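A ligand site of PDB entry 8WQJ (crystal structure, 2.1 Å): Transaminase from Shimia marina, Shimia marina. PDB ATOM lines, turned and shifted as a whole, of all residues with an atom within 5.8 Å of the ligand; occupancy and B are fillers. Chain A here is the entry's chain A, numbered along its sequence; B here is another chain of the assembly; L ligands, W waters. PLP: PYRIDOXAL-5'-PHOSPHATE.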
ATOM      1  N   TRP A  77       0.047  -0.291 -13.905  1.00  0.00           N
ATOM      2  CA  TRP A  77      -0.897  -0.068 -14.995  1.00  0.00           C
ATOM      3  C   TRP A  77      -0.305   0.722 -16.141  1.00  0.00           C
ATOM      4  O   TRP A  77      -1.044   1.352 -16.890  1.00  0.00           O
ATOM      5  CB  TRP A  77      -2.162   0.680 -14.540  1.00  0.00           C
ATOM      6  CG  TRP A  77      -2.808   0.288 -13.244  1.00  0.00           C
ATOM      7  CD1 TRP A  77      -2.396   0.611 -11.979  1.00  0.00           C
ATOM      8  CD2 TRP A  77      -4.035  -0.423 -13.100  1.00  0.00           C
ATOM      9  NE1 TRP A  77      -3.282   0.115 -11.059  1.00  0.00           N
ATOM     10  CE2 TRP A  77      -4.299  -0.512 -11.719  1.00  0.00           C
ATOM     11  CE3 TRP A  77      -4.947  -0.988 -14.008  1.00  0.00           C
ATOM     12  CZ2 TRP A  77      -5.441  -1.152 -11.226  1.00  0.00           C
ATOM     13  CZ3 TRP A  77      -6.073  -1.633 -13.508  1.00  0.00           C
ATOM     14  CH2 TRP A  77      -6.311  -1.710 -12.136  1.00  0.00           C
ATOM     15  N   GLY A 135       3.315  16.465 -14.579  1.00  0.00           N
ATOM     16  CA  GLY A 135       4.311  15.436 -14.382  1.00  0.00           C
ATOM     17  C   GLY A 135       3.692  14.087 -14.094  1.00  0.00           C
ATOM     18  O   GLY A 135       4.375  13.054 -14.130  1.00  0.00           O
ATOM     19  N   SER A 136       2.384  14.082 -13.847  1.00  0.00           N
ATOM     20  CA  SER A 136       1.719  12.911 -13.302  1.00  0.00           C
ATOM     21  C   SER A 136       0.231  13.041 -13.549  1.00  0.00           C
ATOM     22  O   SER A 136      -0.272  14.121 -13.907  1.00  0.00           O
ATOM     23  CB  SER A 136       1.995  12.768 -11.812  1.00  0.00           C
ATOM     24  OG  SER A 136       1.476  13.914 -11.161  1.00  0.00           O
ATOM     25  N   GLY A 137      -0.494  11.942 -13.361  1.00  0.00           N
ATOM     26  CA  GLY A 137      -1.942  11.989 -13.401  1.00  0.00           C
ATOM     27  C   GLY A 137      -2.543  12.800 -12.280  1.00  0.00           C
ATOM     28  O   GLY A 137      -3.639  13.347 -12.432  1.00  0.00           O
ATOM     29  N   SER A 138      -1.861  12.867 -11.128  1.00  0.00           N
ATOM     30  CA  SER A 138      -2.330  13.730 -10.043  1.00  0.00           C
ATOM     31  C   SER A 138      -2.255  15.197 -10.433  1.00  0.00           C
ATOM     32  O   SER A 138      -3.241  15.938 -10.305  1.00  0.00           O
ATOM     33  CB  SER A 138      -1.524  13.493  -8.765  1.00  0.00           C
ATOM     34  OG  SER A 138      -1.635  12.158  -8.350  1.00  0.00           O
ATOM     35  N   GLU A 139      -1.078  15.647 -10.894  1.00  0.00           N
ATOM     36  CA  GLU A 139      -0.926  17.020 -11.352  1.00  0.00           C
ATOM     37  C   GLU A 139      -1.857  17.347 -12.513  1.00  0.00           C
ATOM     38  O   GLU A 139      -2.308  18.489 -12.636  1.00  0.00           O
ATOM     39  CB  GLU A 139       0.522  17.291 -11.753  1.00  0.00           C
ATOM     40  CG  GLU A 139       1.452  17.465 -10.567  1.00  0.00           C
ATOM     41  CD  GLU A 139       2.858  17.895 -10.972  1.00  0.00           C
ATOM     42  OE1 GLU A 139       3.308  17.538 -12.080  1.00  0.00           O
ATOM     43  OE2 GLU A 139       3.515  18.576 -10.149  1.00  0.00           O
ATOM     44  N   ASN A 141      -4.823  16.244 -12.720  1.00  0.00           N
ATOM     45  CA  ASN A 141      -6.123  16.545 -12.116  1.00  0.00           C
ATOM     46  C   ASN A 141      -6.096  17.852 -11.329  1.00  0.00           C
ATOM     47  O   ASN A 141      -7.115  18.529 -11.242  1.00  0.00           O
ATOM     48  CB  ASN A 141      -6.592  15.374 -11.258  1.00  0.00           C
ATOM     49  CG  ASN A 141      -7.116  14.211 -12.118  1.00  0.00           C
ATOM     50  OD1 ASN A 141      -7.812  14.435 -13.120  1.00  0.00           O
ATOM     51  ND2 ASN A 141      -6.746  12.989 -11.756  1.00  0.00           N
ATOM     52  N   TYR A 170     -10.422   6.715  -8.099  1.00  0.00           N
ATOM     53  CA  TYR A 170      -9.028   7.042  -7.834  1.00  0.00           C
ATOM     54  C   TYR A 170      -8.602   8.088  -8.834  1.00  0.00           C
ATOM     55  O   TYR A 170      -8.709   7.883 -10.050  1.00  0.00           O
ATOM     56  CB  TYR A 170      -8.114   5.827  -7.902  1.00  0.00           C
ATOM     57  CG  TYR A 170      -6.746   6.183  -7.361  1.00  0.00           C
ATOM     58  CD1 TYR A 170      -5.772   6.731  -8.193  1.00  0.00           C
ATOM     59  CD2 TYR A 170      -6.453   6.024  -6.004  1.00  0.00           C
ATOM     60  CE1 TYR A 170      -4.537   7.097  -7.697  1.00  0.00           C
ATOM     61  CE2 TYR A 170      -5.212   6.396  -5.504  1.00  0.00           C
ATOM     62  CZ  TYR A 170      -4.260   6.940  -6.363  1.00  0.00           C
ATOM     63  OH  TYR A 170      -3.008   7.315  -5.905  1.00  0.00           O
ATOM     64  N   HIS A 171      -8.112   9.214  -8.330  1.00  0.00           N
ATOM     65  CA  HIS A 171      -7.732  10.317  -9.192  1.00  0.00           C
ATOM     66  C   HIS A 171      -6.392  10.908  -8.796  1.00  0.00           C
ATOM     67  O   HIS A 171      -6.078  12.035  -9.192  1.00  0.00           O
ATOM     68  CB  HIS A 171      -8.812  11.387  -9.201  1.00  0.00           C
ATOM     69  CG  HIS A 171     -10.083  10.937  -9.856  1.00  0.00           C
ATOM     70  ND1 HIS A 171     -10.164  10.634 -11.191  1.00  0.00           N
ATOM     71  CD2 HIS A 171     -11.326  10.721  -9.334  1.00  0.00           C
ATOM     72  CE1 HIS A 171     -11.393  10.257 -11.485  1.00  0.00           C
ATOM     73  NE2 HIS A 171     -12.113  10.307 -10.376  1.00  0.00           N
ATOM     74  N   GLY A 172      -5.587  10.160  -8.022  1.00  0.00           N
ATOM     75  CA  GLY A 172      -4.238  10.562  -7.688  1.00  0.00           C
ATOM     76  C   GLY A 172      -4.086  10.874  -6.204  1.00  0.00           C
ATOM     77  O   GLY A 172      -4.952  10.569  -5.370  1.00  0.00           O
ATOM     78  N   SER A 173      -2.959  11.515  -5.883  1.00  0.00           N
ATOM     79  CA  SER A 173      -2.508  11.609  -4.497  1.00  0.00           C
ATOM     80  C   SER A 173      -2.075  13.004  -4.056  1.00  0.00           C
ATOM     81  O   SER A 173      -1.667  13.157  -2.902  1.00  0.00           O
ATOM     82  CB  SER A 173      -1.359  10.623  -4.263  1.00  0.00           C
ATOM     83  OG  SER A 173      -1.294  10.202  -2.915  1.00  0.00           O
ATOM     84  N   GLU A 243     -13.232   7.775 -14.004  1.00  0.00           N
ATOM     85  CA  GLU A 243     -12.522   6.828 -14.858  1.00  0.00           C
ATOM     86  C   GLU A 243     -13.525   6.060 -15.717  1.00  0.00           C
ATOM     87  O   GLU A 243     -14.546   5.602 -15.199  1.00  0.00           O
ATOM     88  CB  GLU A 243     -11.732   5.815 -14.015  1.00  0.00           C
ATOM     89  CG  GLU A 243     -10.850   6.436 -12.946  1.00  0.00           C
ATOM     90  CD  GLU A 243     -10.686   5.521 -11.766  1.00  0.00           C
ATOM     91  OE1 GLU A 243      -9.784   4.661 -11.836  1.00  0.00           O
ATOM     92  OE2 GLU A 243     -11.449   5.654 -10.793  1.00  0.00           O
ATOM     93  N   ALA A 248      -7.913   1.364  -9.807  1.00  0.00           N
ATOM     94  CA  ALA A 248      -7.491   1.132  -8.422  1.00  0.00           C
ATOM     95  C   ALA A 248      -8.633   0.654  -7.541  1.00  0.00           C
ATOM     96  O   ALA A 248      -8.396  -0.031  -6.548  1.00  0.00           O
ATOM     97  CB  ALA A 248      -6.889   2.420  -7.856  1.00  0.00           C
ATOM     98  N   ASP A 276     -11.075  10.534 -16.692  1.00  0.00           N
ATOM     99  CA  ASP A 276      -9.742  10.267 -16.160  1.00  0.00           C
ATOM    100  C   ASP A 276      -9.202   9.048 -16.916  1.00  0.00           C
ATOM    101  O   ASP A 276      -9.486   7.903 -16.559  1.00  0.00           O
ATOM    102  CB  ASP A 276      -9.782  10.044 -14.649  1.00  0.00           C
ATOM    103  CG  ASP A 276      -8.395  10.026 -14.026  1.00  0.00           C
ATOM    104  OD1 ASP A 276      -7.438   9.684 -14.750  1.00  0.00           O
ATOM    105  OD2 ASP A 276      -8.231  10.350 -12.832  1.00  0.00           O
ATOM    106  N   GLU A 277      -8.418   9.306 -17.963  1.00  0.00           N
ATOM    107  CA  GLU A 277      -7.852   8.278 -18.835  1.00  0.00           C
ATOM    108  C   GLU A 277      -6.444   7.869 -18.432  1.00  0.00           C
ATOM    109  O   GLU A 277      -5.726   7.261 -19.251  1.00  0.00           O
ATOM    110  CB  GLU A 277      -7.829   8.779 -20.281  1.00  0.00           C
ATOM    111  CG  GLU A 277      -9.184   9.124 -20.844  1.00  0.00           C
ATOM    112  CD  GLU A 277      -9.906   7.920 -21.359  1.00  0.00           C
ATOM    113  OE1 GLU A 277      -9.308   6.830 -21.289  1.00  0.00           O
ATOM    114  OE2 GLU A 277     -11.055   8.062 -21.827  1.00  0.00           O
ATOM    115  N   VAL A 278      -6.012   8.192 -17.214  1.00  0.00           N
ATOM    116  CA  VAL A 278      -4.649   7.879 -16.791  1.00  0.00           C
ATOM    117  C   VAL A 278      -4.357   6.386 -16.908  1.00  0.00           C
ATOM    118  O   VAL A 278      -3.274   5.980 -17.354  1.00  0.00           O
ATOM    119  CB  VAL A 278      -4.405   8.394 -15.356  1.00  0.00           C
ATOM    120  CG1 VAL A 278      -3.109   7.809 -14.803  1.00  0.00           C
ATOM    121  CG2 VAL A 278      -4.368   9.908 -15.349  1.00  0.00           C
ATOM    122  N   ILE A 279      -5.295   5.540 -16.507  1.00  0.00           N
ATOM    123  CA  ILE A 279      -5.138   4.097 -16.700  1.00  0.00           C
ATOM    124  C   ILE A 279      -5.690   3.641 -18.051  1.00  0.00           C
ATOM    125  O   ILE A 279      -5.019   2.911 -18.795  1.00  0.00           O
ATOM    126  CB  ILE A 279      -5.804   3.318 -15.554  1.00  0.00           C
ATOM    127  CG1 ILE A 279      -4.912   3.320 -14.303  1.00  0.00           C
ATOM    128  CG2 ILE A 279      -6.143   1.914 -16.025  1.00  0.00           C
ATOM    129  CD1 ILE A 279      -5.500   2.558 -13.115  1.00  0.00           C
ATOM    130  N   ALA A 304      -1.566  10.089 -18.209  1.00  0.00           N
ATOM    131  CA  ALA A 304      -0.230   9.792 -17.706  1.00  0.00           C
ATOM    132  C   ALA A 304       0.023   8.308 -17.977  1.00  0.00           C
ATOM    133  O   ALA A 304      -0.408   7.787 -19.020  1.00  0.00           O
ATOM    134  CB  ALA A 304      -0.072  10.121 -16.208  1.00  0.00           C
ATOM    135  N   LYS A 305       0.689   7.616 -17.045  1.00  0.00           N
ATOM    136  CA  LYS A 305       1.005   6.191 -17.158  1.00  0.00           C
ATOM    137  C   LYS A 305       1.329   5.759 -18.596  1.00  0.00           C
ATOM    138  O   LYS A 305       2.464   5.914 -19.041  1.00  0.00           O
ATOM    139  CB  LYS A 305      -0.142   5.365 -16.561  1.00  0.00           C
ATOM    140  CG  LYS A 305      -0.297   5.523 -15.032  1.00  0.00           C
ATOM    141  CD  LYS A 305      -1.210   4.468 -14.431  1.00  0.00           C
ATOM    142  CE  LYS A 305      -1.223   4.516 -12.886  1.00  0.00           C
ATOM    143  NZ  LYS A 305      -2.238   5.498 -12.371  1.00  0.00           N
ATOM    144  N   PHE B 105       5.256   0.697  -4.767  1.00  0.00           N
ATOM    145  CA  PHE B 105       3.981   0.519  -4.058  1.00  0.00           C
ATOM    146  C   PHE B 105       3.798  -0.907  -3.532  1.00  0.00           C
ATOM    147  O   PHE B 105       3.096  -1.109  -2.520  1.00  0.00           O
ATOM    148  CB  PHE B 105       2.789   0.808  -4.984  1.00  0.00           C
ATOM    149  CG  PHE B 105       2.598   2.275  -5.357  1.00  0.00           C
ATOM    150  CD1 PHE B 105       3.619   3.002  -5.950  1.00  0.00           C
ATOM    151  CD2 PHE B 105       1.374   2.874  -5.187  1.00  0.00           C
ATOM    152  CE1 PHE B 105       3.417   4.330  -6.316  1.00  0.00           C
ATOM    153  CE2 PHE B 105       1.166   4.195  -5.557  1.00  0.00           C
ATOM    154  CZ  PHE B 105       2.202   4.921  -6.128  1.00  0.00           C
ATOM    155  N   GLU B 139       4.370  18.680  -6.253  1.00  0.00           N
ATOM    156  CA  GLU B 139       3.922  17.444  -5.637  1.00  0.00           C
ATOM    157  C   GLU B 139       4.658  17.163  -4.315  1.00  0.00           C
ATOM    158  O   GLU B 139       4.111  16.492  -3.431  1.00  0.00           O
ATOM    159  CB  GLU B 139       4.098  16.273  -6.605  1.00  0.00           C
ATOM    160  CG  GLU B 139       3.166  16.316  -7.775  1.00  0.00           C
ATOM    161  CD  GLU B 139       3.253  15.066  -8.645  1.00  0.00           C
ATOM    162  OE1 GLU B 139       4.358  14.480  -8.732  1.00  0.00           O
ATOM    163  OE2 GLU B 139       2.227  14.678  -9.223  1.00  0.00           O
ATOM    164  N   GLY B 335       1.157   8.988  -2.460  1.00  0.00           N
ATOM    165  CA  GLY B 335       2.294   8.761  -3.325  1.00  0.00           C
ATOM    166  C   GLY B 335       1.894   8.681  -4.779  1.00  0.00           C
ATOM    167  O   GLY B 335       0.714   8.583  -5.123  1.00  0.00           O
ATOM    168  N   TYR B 336       2.886   8.704  -5.649  1.00  0.00           N
ATOM    169  CA  TYR B 336       2.640   8.902  -7.078  1.00  0.00           C
ATOM    170  C   TYR B 336       3.224   7.751  -7.877  1.00  0.00           C
ATOM    171  O   TYR B 336       4.239   7.161  -7.492  1.00  0.00           O
ATOM    172  CB  TYR B 336       3.224  10.230  -7.550  1.00  0.00           C
ATOM    173  CG  TYR B 336       2.928  11.376  -6.622  1.00  0.00           C
ATOM    174  CD1 TYR B 336       1.717  12.035  -6.680  1.00  0.00           C
ATOM    175  CD2 TYR B 336       3.858  11.802  -5.685  1.00  0.00           C
ATOM    176  CE1 TYR B 336       1.435  13.115  -5.835  1.00  0.00           C
ATOM    177  CE2 TYR B 336       3.588  12.867  -4.814  1.00  0.00           C
ATOM    178  CZ  TYR B 336       2.378  13.514  -4.899  1.00  0.00           C
ATOM    179  OH  TYR B 336       2.121  14.578  -4.046  1.00  0.00           O
ATOM    180  N   THR B 337       2.586   7.443  -9.005  1.00  0.00           N
ATOM    181  CA  THR B 337       3.048   6.324  -9.830  1.00  0.00           C
ATOM    182  C   THR B 337       4.542   6.455 -10.108  1.00  0.00           C
ATOM    183  O   THR B 337       5.287   5.462 -10.047  1.00  0.00           O
ATOM    184  CB  THR B 337       2.244   6.258 -11.137  1.00  0.00           C
ATOM    185  OG1 THR B 337       0.870   5.978 -10.847  1.00  0.00           O
ATOM    186  CG2 THR B 337       2.781   5.167 -12.079  1.00  0.00           C
ATOM    187  N   TYR B 338       5.020   7.672 -10.353  1.00  0.00           N
ATOM    188  CA  TYR B 338       6.414   7.855 -10.714  1.00  0.00           C
ATOM    189  C   TYR B 338       7.313   8.208  -9.529  1.00  0.00           C
ATOM    190  O   TYR B 338       8.492   8.512  -9.737  1.00  0.00           O
ATOM    191  CB  TYR B 338       6.552   8.908 -11.825  1.00  0.00           C
ATOM    192  CG  TYR B 338       5.917   8.420 -13.104  1.00  0.00           C
ATOM    193  CD1 TYR B 338       6.094   7.117 -13.533  1.00  0.00           C
ATOM    194  CD2 TYR B 338       5.078   9.246 -13.850  1.00  0.00           C
ATOM    195  CE1 TYR B 338       5.509   6.663 -14.690  1.00  0.00           C
ATOM    196  CE2 TYR B 338       4.472   8.790 -15.017  1.00  0.00           C
ATOM    197  CZ  TYR B 338       4.706   7.493 -15.425  1.00  0.00           C
ATOM    198  OH  TYR B 338       4.117   7.025 -16.580  1.00  0.00           O
HETATM  199  N1  PLP L   1      -6.048   8.888 -12.135  1.00  0.00           N
HETATM  200  C2  PLP L   1      -6.137   7.517 -12.259  1.00  0.00           C
HETATM  201  C2A PLP L   1      -7.387   6.893 -12.821  1.00  0.00           C
HETATM  202  C3  PLP L   1      -5.069   6.713 -11.856  1.00  0.00           C
HETATM  203  O3  PLP L   1      -5.146   5.357 -11.954  1.00  0.00           O
HETATM  204  C4  PLP L   1      -3.912   7.277 -11.347  1.00  0.00           C
HETATM  205  C4A PLP L   1      -2.681   6.400 -11.351  1.00  0.00           C
HETATM  206  C5  PLP L   1      -3.826   8.662 -11.237  1.00  0.00           C
HETATM  207  C6  PLP L   1      -4.893   9.469 -11.622  1.00  0.00           C
HETATM  208  C5A PLP L   1      -2.595   9.317 -10.668  1.00  0.00           C
HETATM  209  O4P PLP L   1      -1.487   9.253 -11.537  1.00  0.00           O
HETATM  210  P   PLP L   1      -0.082   9.569 -10.843  1.00  0.00           P
HETATM  211  O1P PLP L   1      -0.189  10.912 -10.177  1.00  0.00           O
HETATM  212  O2P PLP L   1       0.236   8.471  -9.822  1.00  0.00           O
HETATM  213  O3P PLP L   1       0.974   9.576 -11.929  1.00  0.00           O
HETATM  214  O   HOH W   1       3.391   9.910 -10.921  1.00  0.00           O
HETATM  215  O   HOH W   2      -7.371   3.780 -10.718  1.00  0.00           O
HETATM  216  O   HOH W   3      -1.205   8.653  -7.495  1.00  0.00           O
HETATM  217  O   HOH W   4       1.653   8.072 -14.151  1.00  0.00           O
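Merely in contact with the ligand: Ile 279 (3.1 Å), Tyr 170 (3.2 Å), Ser 136 (3.3 Å), Glu 243 (3.4 Å), His 171 (3.5 Å), Val 278 (3.6 Å), Gly 172 (3.6 Å), Tyr 336 of chain B (3.6 Å) and Asn 141 (3.98 Å).
Hydrophobic or aromatic side chains within 4 Å of the ligand: Tyr 170, Val 278 and Ile 279.
14 residues have an atom within 4 Å of the ligand: Ser 136, Gly 137, Ser 138, Asn 141, Tyr 170, His 171, Gly 172, Glu 243, Asp 276, Val 278, Ile 279, Lys 305, Tyr 336 of chain B and Thr 337 of chain B.
The side-chain amino group (NZ) of Lys 305 sits close to the side-chain hydroxyl (OG1) of Thr 337 of chain B (3.5 Å).
O of Lys 305 sits at hydrogen-bond distance from OH of Tyr 338 of chain B (3.2 Å).
The backbone NH (N) of Ser 138 sits close to the side-chain hydroxyl (OG) of Ser 136.
The side-chain hydroxyl (OG) of Ser 138 lies within hydrogen-bond range of the backbone NH (N) of Ser 173 (2.9 Å).
The side-chain carboxylate (OD2) of Asp 276 sits at hydrogen-bond distance from a ring nitrogen (ND1) of His 171, 2.6 Å away.
The side-chain amide nitrogen (ND2) of Asn 141 sits at hydrogen-bond distance from the backbone carbonyl oxygen (O) of Gly 137 (3.2 Å).
The side-chain hydroxyl of Ser 136 is in hydrogen-bond range of the backbone NH of Glu 139 of chain A (3.1 Å).
The backbone carbonyl oxygen of Glu 139 of chain B sits at hydrogen-bond distance from the side-chain hydroxyl of Tyr 336 of chain B.
The side-chain amino group (NZ) of Lys 305 is bonded to a carbon (C4A) of the ligand, 1.4 Å away.
The backbone NH (N) of Ser 138 sits at hydrogen-bond distance from an oxygen (O1P) of the ligand, at 2.7 Å.
O1P of the ligand sits at hydrogen-bond distance from OG of Ser 138.
N of Thr 337 of chain B lies within hydrogen-bond range of O2P of the ligand (2.7 Å).
OG1 of Thr 337 of chain B is in hydrogen-bond range of O2P of the ligand, 2.8 Å away.
The side-chain carboxylate (OD2) of Asp 276 sits at hydrogen-bond distance from a nitrogen (N1) of the ligand, at 2.7 Å.
The backbone NH of Gly 137 is in hydrogen-bond range of an oxygen (O3P) of the ligand (3.1 Å).
Water W1 lies within hydrogen-bond range of an oxygen (O3P) of the ligand, the backbone NH (N) of Tyr 338 of chain B and the backbone NH (N) of Thr 337 of chain B.
Water W3 lies within hydrogen-bond range of O2P of the ligand (2.7 Å), OH of Tyr 170 (2.8 Å) and O of Gly 335 of chain B (3.1 Å).
Water W4 bridges an oxygen (O3P) of the ligand (2.8 Å) and the backbone NH (N) of Lys 305 (3.1 Å).
Water W2 lies within hydrogen-bond range of the backbone NH (N) of Ala 248 (2.6 Å), the side-chain carboxylate (OE1) of Glu 243 (2.8 Å) and an oxygen (O3) of the ligand (3.0 Å).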
